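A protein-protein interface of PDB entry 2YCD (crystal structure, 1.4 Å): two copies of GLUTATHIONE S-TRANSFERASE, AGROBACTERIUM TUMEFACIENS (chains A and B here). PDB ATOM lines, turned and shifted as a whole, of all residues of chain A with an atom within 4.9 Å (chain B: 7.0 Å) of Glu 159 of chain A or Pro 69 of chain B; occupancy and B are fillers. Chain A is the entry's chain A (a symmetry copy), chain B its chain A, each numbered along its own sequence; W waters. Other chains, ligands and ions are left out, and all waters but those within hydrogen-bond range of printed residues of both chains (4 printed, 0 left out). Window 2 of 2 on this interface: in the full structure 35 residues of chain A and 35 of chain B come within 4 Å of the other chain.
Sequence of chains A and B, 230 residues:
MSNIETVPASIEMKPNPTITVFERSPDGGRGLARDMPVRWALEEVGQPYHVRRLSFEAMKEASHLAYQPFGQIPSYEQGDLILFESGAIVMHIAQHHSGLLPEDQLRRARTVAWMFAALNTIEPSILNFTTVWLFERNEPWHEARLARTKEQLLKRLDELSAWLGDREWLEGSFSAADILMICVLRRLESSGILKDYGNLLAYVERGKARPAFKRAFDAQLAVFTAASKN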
ATOM      1  N   TRP A 114      30.989  -9.231  30.259  1.00  0.00           N
ATOM      2  CA  TRP A 114      29.683  -9.614  29.733  1.00  0.00           C
ATOM      3  C   TRP A 114      28.800 -10.293  30.779  1.00  0.00           C
ATOM      4  O   TRP A 114      27.581 -10.153  30.720  1.00  0.00           O
ATOM      5  CB  TRP A 114      29.831 -10.462  28.449  1.00  0.00           C
ATOM      6  CG  TRP A 114      30.100  -9.574  27.258  1.00  0.00           C
ATOM      7  CD1 TRP A 114      31.268  -9.454  26.573  1.00  0.00           C
ATOM      8  CD2 TRP A 114      29.184  -8.640  26.671  1.00  0.00           C
ATOM      9  NE1 TRP A 114      31.125  -8.517  25.557  1.00  0.00           N
ATOM     10  CE2 TRP A 114      29.849  -8.012  25.601  1.00  0.00           C
ATOM     11  CE3 TRP A 114      27.848  -8.324  26.907  1.00  0.00           C
ATOM     12  CZ2 TRP A 114      29.227  -7.035  24.802  1.00  0.00           C
ATOM     13  CZ3 TRP A 114      27.233  -7.348  26.119  1.00  0.00           C
ATOM     14  CH2 TRP A 114      27.915  -6.735  25.072  1.00  0.00           C
ATOM     15  N   LYS A 155      15.777   0.225  23.011  1.00  0.00           N
ATOM     16  CA  LYS A 155      17.069   0.864  22.795  1.00  0.00           C
ATOM     17  C   LYS A 155      18.236  -0.049  23.228  1.00  0.00           C
ATOM     18  O   LYS A 155      19.214  -0.205  22.503  1.00  0.00           O
ATOM     19  CB  LYS A 155      17.102   2.217  23.513  1.00  0.00           C
ATOM     20  CG  LYS A 155      18.414   2.963  23.369  1.00  0.00           C
ATOM     21  CD  LYS A 155      18.294   4.380  23.910  1.00  0.00           C
ATOM     22  CE  LYS A 155      19.603   5.148  23.747  1.00  0.00           C
ATOM     23  NZ  LYS A 155      20.696   4.603  24.609  1.00  0.00           N
ATOM     24  N   ARG A 156      18.125  -0.662  24.405  1.00  0.00           N
ATOM     25  CA  ARG A 156      19.162  -1.586  24.870  1.00  0.00           C
ATOM     26  C   ARG A 156      19.271  -2.832  23.993  1.00  0.00           C
ATOM     27  O   ARG A 156      20.370  -3.326  23.750  1.00  0.00           O
ATOM     28  CB  ARG A 156      18.904  -2.004  26.323  1.00  0.00           C
ATOM     29  CG  ARG A 156      19.146  -0.901  27.320  1.00  0.00           C
ATOM     30  CD  ARG A 156      20.635  -0.615  27.530  1.00  0.00           C
ATOM     31  NE  ARG A 156      20.794   0.453  28.505  1.00  0.00           N
ATOM     32  CZ  ARG A 156      21.207   1.684  28.231  1.00  0.00           C
ATOM     33  NH1 ARG A 156      21.541   2.032  26.995  1.00  0.00           N
ATOM     34  NH2 ARG A 156      21.300   2.573  29.216  1.00  0.00           N
ATOM     35  N   LEU A 157      18.139  -3.344  23.509  1.00  0.00           N
ATOM     36  CA  LEU A 157      18.164  -4.482  22.603  1.00  0.00           C
ATOM     37  C   LEU A 157      18.760  -4.116  21.235  1.00  0.00           C
ATOM     38  O   LEU A 157      19.503  -4.900  20.661  1.00  0.00           O
ATOM     39  CB  LEU A 157      16.767  -5.104  22.446  1.00  0.00           C
ATOM     40  CG  LEU A 157      16.145  -5.683  23.731  1.00  0.00           C
ATOM     41  CD1 LEU A 157      14.742  -6.207  23.470  1.00  0.00           C
ATOM     42  CD2 LEU A 157      16.993  -6.810  24.319  1.00  0.00           C
ATOM     43  N   ASP A 158      18.453  -2.913  20.754  1.00  0.00           N
ATOM     44  CA  ASP A 158      19.105  -2.384  19.543  1.00  0.00           C
ATOM     45  C   ASP A 158      20.617  -2.422  19.735  1.00  0.00           C
ATOM     46  O   ASP A 158      21.355  -2.898  18.885  1.00  0.00           O
ATOM     47  CB  ASP A 158      18.722  -0.922  19.258  1.00  0.00           C
ATOM     48  CG  ASP A 158      17.285  -0.745  18.774  1.00  0.00           C
ATOM     49  OD1 ASP A 158      16.645  -1.726  18.335  1.00  0.00           O
ATOM     50  OD2 ASP A 158      16.806   0.414  18.832  1.00  0.00           O
ATOM     51  N   GLU A 159      21.080  -1.898  20.868  1.00  0.00           N
ATOM     52  CA  GLU A 159      22.511  -1.837  21.154  1.00  0.00           C
ATOM     53  C   GLU A 159      23.154  -3.227  21.257  1.00  0.00           C
ATOM     54  O   GLU A 159      24.234  -3.484  20.701  1.00  0.00           O
ATOM     55  CB  GLU A 159      22.743  -1.015  22.433  1.00  0.00           C
ATOM     56  CG  GLU A 159      22.457   0.483  22.212  1.00  0.00           C
ATOM     57  CD  GLU A 159      22.050   1.240  23.465  1.00  0.00           C
ATOM     58  OE1 GLU A 159      21.981   0.659  24.570  1.00  0.00           O
ATOM     59  OE2 GLU A 159      21.791   2.456  23.361  1.00  0.00           O
ATOM     60  N   LEU A 160      22.495  -4.138  21.969  1.00  0.00           N
ATOM     61  CA  LEU A 160      23.024  -5.484  22.118  1.00  0.00           C
ATOM     62  C   LEU A 160      23.078  -6.224  20.779  1.00  0.00           C
ATOM     63  O   LEU A 160      24.038  -6.932  20.471  1.00  0.00           O
ATOM     64  CB  LEU A 160      22.161  -6.277  23.113  1.00  0.00           C
ATOM     65  CG  LEU A 160      22.631  -7.708  23.388  1.00  0.00           C
ATOM     66  CD1 LEU A 160      24.005  -7.726  24.043  1.00  0.00           C
ATOM     67  CD2 LEU A 160      21.619  -8.465  24.258  1.00  0.00           C
ATOM     68  N   SER A 161      22.019  -6.061  19.994  1.00  0.00           N
ATOM     69  CA  SER A 161      21.917  -6.712  18.683  1.00  0.00           C
ATOM     70  C   SER A 161      23.001  -6.211  17.724  1.00  0.00           C
ATOM     71  O   SER A 161      23.637  -7.009  17.028  1.00  0.00           O
ATOM     72  CB  SER A 161      20.527  -6.445  18.117  1.00  0.00           C
ATOM     73  OG  SER A 161      20.410  -6.977  16.802  1.00  0.00           O
ATOM     74  N   ALA A 162      23.231  -4.900  17.736  1.00  0.00           N
ATOM     75  CA  ALA A 162      24.234  -4.316  16.854  1.00  0.00           C
ATOM     76  C   ALA A 162      25.606  -4.818  17.247  1.00  0.00           C
ATOM     77  O   ALA A 162      26.452  -5.133  16.401  1.00  0.00           O
ATOM     78  CB  ALA A 162      24.183  -2.808  16.924  1.00  0.00           C
ATOM     79  N   TRP A 163      25.849  -4.897  18.544  1.00  0.00           N
ATOM     80  CA  TRP A 163      27.142  -5.343  18.974  1.00  0.00           C
ATOM     81  C   TRP A 163      27.373  -6.835  18.642  1.00  0.00           C
ATOM     82  O   TRP A 163      28.461  -7.225  18.191  1.00  0.00           O
ATOM     83  CB  TRP A 163      27.362  -5.009  20.458  1.00  0.00           C
ATOM     84  CG  TRP A 163      28.725  -5.382  20.854  1.00  0.00           C
ATOM     85  CD1 TRP A 163      29.850  -4.601  20.830  1.00  0.00           C
ATOM     86  CD2 TRP A 163      29.138  -6.678  21.267  1.00  0.00           C
ATOM     87  NE1 TRP A 163      30.936  -5.341  21.224  1.00  0.00           N
ATOM     88  CE2 TRP A 163      30.524  -6.624  21.488  1.00  0.00           C
ATOM     89  CE3 TRP A 163      28.470  -7.889  21.456  1.00  0.00           C
ATOM     90  CZ2 TRP A 163      31.254  -7.733  21.914  1.00  0.00           C
ATOM     91  CZ3 TRP A 163      29.199  -8.978  21.871  1.00  0.00           C
ATOM     92  CH2 TRP A 163      30.567  -8.895  22.102  1.00  0.00           C
ATOM     93  N   HIS B  64      32.240   6.001  20.367  1.00  0.00           N
ATOM     94  CA  HIS B  64      32.241   5.585  21.762  1.00  0.00           C
ATOM     95  C   HIS B  64      31.760   4.140  21.945  1.00  0.00           C
ATOM     96  O   HIS B  64      32.147   3.466  22.897  1.00  0.00           O
ATOM     97  CB  HIS B  64      31.422   6.548  22.611  1.00  0.00           C
ATOM     98  CG  HIS B  64      31.494   6.245  24.071  1.00  0.00           C
ATOM     99  ND1 HIS B  64      30.382   6.203  24.879  1.00  0.00           N
ATOM    100  CD2 HIS B  64      32.556   5.962  24.865  1.00  0.00           C
ATOM    101  CE1 HIS B  64      30.754   5.904  26.113  1.00  0.00           C
ATOM    102  NE2 HIS B  64      32.063   5.751  26.130  1.00  0.00           N
ATOM    103  N   LEU B  65      30.932   3.665  21.024  1.00  0.00           N
ATOM    104  CA  LEU B  65      30.420   2.297  21.088  1.00  0.00           C
ATOM    105  C   LEU B  65      31.521   1.246  20.994  1.00  0.00           C
ATOM    106  O   LEU B  65      31.331   0.112  21.443  1.00  0.00           O
ATOM    107  CB  LEU B  65      29.356   2.067  20.008  1.00  0.00           C
ATOM    108  CG  LEU B  65      28.138   2.980  20.163  1.00  0.00           C
ATOM    109  CD1 LEU B  65      27.177   2.832  18.990  1.00  0.00           C
ATOM    110  CD2 LEU B  65      27.414   2.702  21.480  1.00  0.00           C
ATOM    111  N   ALA B  66      32.671   1.598  20.423  1.00  0.00           N
ATOM    112  CA  ALA B  66      33.808   0.682  20.389  1.00  0.00           C
ATOM    113  C   ALA B  66      34.406   0.457  21.774  1.00  0.00           C
ATOM    114  O   ALA B  66      35.258  -0.418  21.959  1.00  0.00           O
ATOM    115  CB  ALA B  66      34.891   1.197  19.434  1.00  0.00           C
ATOM    116  N   TYR B  67      33.976   1.262  22.741  1.00  0.00           N
ATOM    117  CA  TYR B  67      34.494   1.168  24.108  1.00  0.00           C
ATOM    118  C   TYR B  67      33.422   0.700  25.077  1.00  0.00           C
ATOM    119  O   TYR B  67      33.699  -0.055  26.019  1.00  0.00           O
ATOM    120  CB  TYR B  67      35.033   2.528  24.549  1.00  0.00           C
ATOM    121  CG  TYR B  67      36.192   2.976  23.696  1.00  0.00           C
ATOM    122  CD1 TYR B  67      35.987   3.714  22.537  1.00  0.00           C
ATOM    123  CD2 TYR B  67      37.497   2.627  24.036  1.00  0.00           C
ATOM    124  CE1 TYR B  67      37.058   4.123  21.755  1.00  0.00           C
ATOM    125  CE2 TYR B  67      38.568   3.024  23.259  1.00  0.00           C
ATOM    126  CZ  TYR B  67      38.342   3.764  22.118  1.00  0.00           C
ATOM    127  OH  TYR B  67      39.414   4.157  21.347  1.00  0.00           O
ATOM    128  N   GLN B  68      32.202   1.166  24.844  1.00  0.00           N
ATOM    129  CA  GLN B  68      31.078   0.854  25.709  1.00  0.00           C
ATOM    130  C   GLN B  68      29.856   0.684  24.799  1.00  0.00           C
ATOM    131  O   GLN B  68      29.353   1.662  24.250  1.00  0.00           O
ATOM    132  CB  GLN B  68      30.895   1.959  26.759  1.00  0.00           C
ATOM    133  CG  GLN B  68      30.508   1.462  28.155  1.00  0.00           C
ATOM    134  CD  GLN B  68      29.048   1.086  28.263  1.00  0.00           C
ATOM    135  OE1 GLN B  68      28.279   1.230  27.312  1.00  0.00           O
ATOM    136  NE2 GLN B  68      28.647   0.628  29.437  1.00  0.00           N
ATOM    137  N   PRO B  69      29.409  -0.565  24.603  1.00  0.00           N
ATOM    138  CA  PRO B  69      28.391  -0.847  23.579  1.00  0.00           C
ATOM    139  C   PRO B  69      27.021  -0.251  23.845  1.00  0.00           C
ATOM    140  O   PRO B  69      26.173  -0.280  22.949  1.00  0.00           O
ATOM    141  CB  PRO B  69      28.269  -2.377  23.599  1.00  0.00           C
ATOM    142  CG  PRO B  69      29.461  -2.883  24.293  1.00  0.00           C
ATOM    143  CD  PRO B  69      29.982  -1.795  25.182  1.00  0.00           C
ATOM    144  N   PHE B  70      26.795   0.264  25.052  1.00  0.00           N
ATOM    145  CA  PHE B  70      25.519   0.864  25.402  1.00  0.00           C
ATOM    146  C   PHE B  70      25.623   2.381  25.551  1.00  0.00           C
ATOM    147  O   PHE B  70      24.691   3.026  26.053  1.00  0.00           O
ATOM    148  CB  PHE B  70      25.003   0.176  26.678  1.00  0.00           C
ATOM    149  CG  PHE B  70      24.931  -1.320  26.522  1.00  0.00           C
ATOM    150  CD1 PHE B  70      23.910  -1.887  25.798  1.00  0.00           C
ATOM    151  CD2 PHE B  70      25.937  -2.143  27.004  1.00  0.00           C
ATOM    152  CE1 PHE B  70      23.854  -3.249  25.584  1.00  0.00           C
ATOM    153  CE2 PHE B  70      25.891  -3.521  26.807  1.00  0.00           C
ATOM    154  CZ  PHE B  70      24.831  -4.080  26.091  1.00  0.00           C
ATOM    155  N   GLY B  71      26.758   2.938  25.116  1.00  0.00           N
ATOM    156  CA  GLY B  71      26.955   4.381  25.102  1.00  0.00           C
ATOM    157  C   GLY B  71      26.999   5.024  26.476  1.00  0.00           C
ATOM    158  O   GLY B  71      26.579   6.178  26.640  1.00  0.00           O
ATOM    159  N   GLN B  72      27.509   4.285  27.462  1.00  0.00           N
ATOM    160  CA  GLN B  72      27.560   4.770  28.830  1.00  0.00           C
ATOM    161  C   GLN B  72      29.003   4.831  29.324  1.00  0.00           C
ATOM    162  O   GLN B  72      29.923   4.361  28.653  1.00  0.00           O
ATOM    163  CB  GLN B  72      26.720   3.868  29.744  1.00  0.00           C
ATOM    164  CG  GLN B  72      25.228   3.937  29.414  1.00  0.00           C
ATOM    165  CD  GLN B  72      24.355   3.370  30.496  1.00  0.00           C
ATOM    166  OE1 GLN B  72      24.456   2.185  30.827  1.00  0.00           O
ATOM    167  NE2 GLN B  72      23.467   4.202  31.040  1.00  0.00           N
ATOM    168  N   PHE B  84      34.299  -2.879  29.895  1.00  0.00           N
ATOM    169  CA  PHE B  84      33.217  -2.047  30.394  1.00  0.00           C
ATOM    170  C   PHE B  84      32.559  -2.791  31.558  1.00  0.00           C
ATOM    171  O   PHE B  84      32.966  -3.920  31.875  1.00  0.00           O
ATOM    172  CB  PHE B  84      32.252  -1.625  29.272  1.00  0.00           C
ATOM    173  CG  PHE B  84      31.356  -2.715  28.788  1.00  0.00           C
ATOM    174  CD1 PHE B  84      31.848  -3.706  27.962  1.00  0.00           C
ATOM    175  CD2 PHE B  84      30.022  -2.749  29.152  1.00  0.00           C
ATOM    176  CE1 PHE B  84      31.009  -4.729  27.483  1.00  0.00           C
ATOM    177  CE2 PHE B  84      29.175  -3.763  28.696  1.00  0.00           C
ATOM    178  CZ  PHE B  84      29.678  -4.763  27.874  1.00  0.00           C
HETATM  179  O   HOH W   1      20.535   2.846  32.076  1.00  0.00           O
HETATM  180  O   HOH W   2      23.851   4.233  22.916  1.00  0.00           O
HETATM  181  O   HOH W   3      22.630   4.902  27.278  1.00  0.00           O
HETATM  182  O   HOH W   4      25.903  -1.262  20.405  1.00  0.00           O
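Of the printed residues of chain B, Trp 114 of chain A touches Phe 84 (3.8 Å). Glu 159 of chain A touches just these residues of chain B: Pro 69 and Phe 70. Printed residues of chain B within 4 Å of Leu 160 of chain A: Phe 70 (3.96 Å). Of the printed residues of chain A, Phe 70 of chain B touches Arg 156 (3.4 Å), Glu 159 (3.4 Å) and Leu 160 (3.96 Å). Of the printed residues of chain A, Gln 72 of chain B touches Arg 156 (3.3 Å). The nearest residue of chain B that does not touch Glu 159 of chain A is Gly 71 of chain B (5.3 Å). The nearest residue of chain A that does not touch Pro 69 of chain B is Trp 114 of chain A (4.2 Å).
Printed residues of chain B that touch a printed residue of chain A: Pro 69, Phe 70, Gln 72 and Phe 84. Printed residues of chain A that touch a printed residue of chain B: Trp 114, Arg 156, Glu 159, Leu 160 and Trp 163. Hydrophobic or aromatic side chains of chain A within 4 Å of the printed part of chain B: Trp 114 and Trp 163. Among the printed residues, 7 pairs touch across the chains. Among the printed residues, no Asp or Glu carboxylate lies within 4 Å of a Lys or Arg side-chain nitrogen of the other chain.
Among the printed residues, merely in contact across the chains: Trp 114 of chain A with Phe 84 of chain B (3.8 Å), Glu 159 of chain A with Pro 69 of chain B (3.5 Å), Glu 159 of chain A with Phe 70 of chain B (3.4 Å), Leu 160 of chain A with Phe 70 of chain B (3.96 Å) and Trp 163 of chain A with Pro 69 of chain B (3.9 Å).
No position is printed for both chains. Of the 7 pairs that touch across the chains among the printed residues, none has its exchanged pair printed and touching as well.
The backbone NH (N) of Phe 70 of chain B is in hydrogen-bond range of the side-chain amide oxygen (OE1) of Gln 68 of chain B (2.9 Å). The backbone NH (N) of Gln 72 of chain B sits at hydrogen-bond distance from the side-chain amide oxygen (OE1) of Gln 68 of chain B, 3.2 Å away. The side-chain amino group (NZ) of Lys 155 of chain A is in salt-bridge range of the side-chain carboxylate (OE2) of Glu 159 of chain A, 2.7 Å away. The guanidinium group (NH1) of Arg 156 of chain A is in salt-bridge range of the side-chain carboxylate (OE1) of Glu 159 of chain A.
Water W4 bridges the backbone carbonyl oxygen (O) of Pro 69 of chain B (2.7 Å) and the backbone carbonyl oxygen (O) of Glu 159 of chain A (2.8 Å). Water W2 lies within hydrogen-bond range of OE2 of Glu 159 of chain A and O of Phe 70 of chain B. Water W1 bridges the guanidinium group of Arg 156 of chain A (3.0 Å) and the side-chain amide nitrogen of Gln 72 of chain B (3.4 Å). Water W3 lies within hydrogen-bond range of the backbone carbonyl oxygen (O) of Phe 70 of chain B, the guanidinium group (NH1) of Arg 156 of chain A and the side-chain amino group (NZ) of Lys 155 of chain A.
The guanidinium group (NH1) of Arg 156 of chain A is in hydrogen-bond range of the backbone carbonyl oxygen (O) of Phe 70 of chain B, 3.4 Å away. NE2 of Gln 72 of chain B sits close to NH2 of Arg 156 of chain A (3.3 Å).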
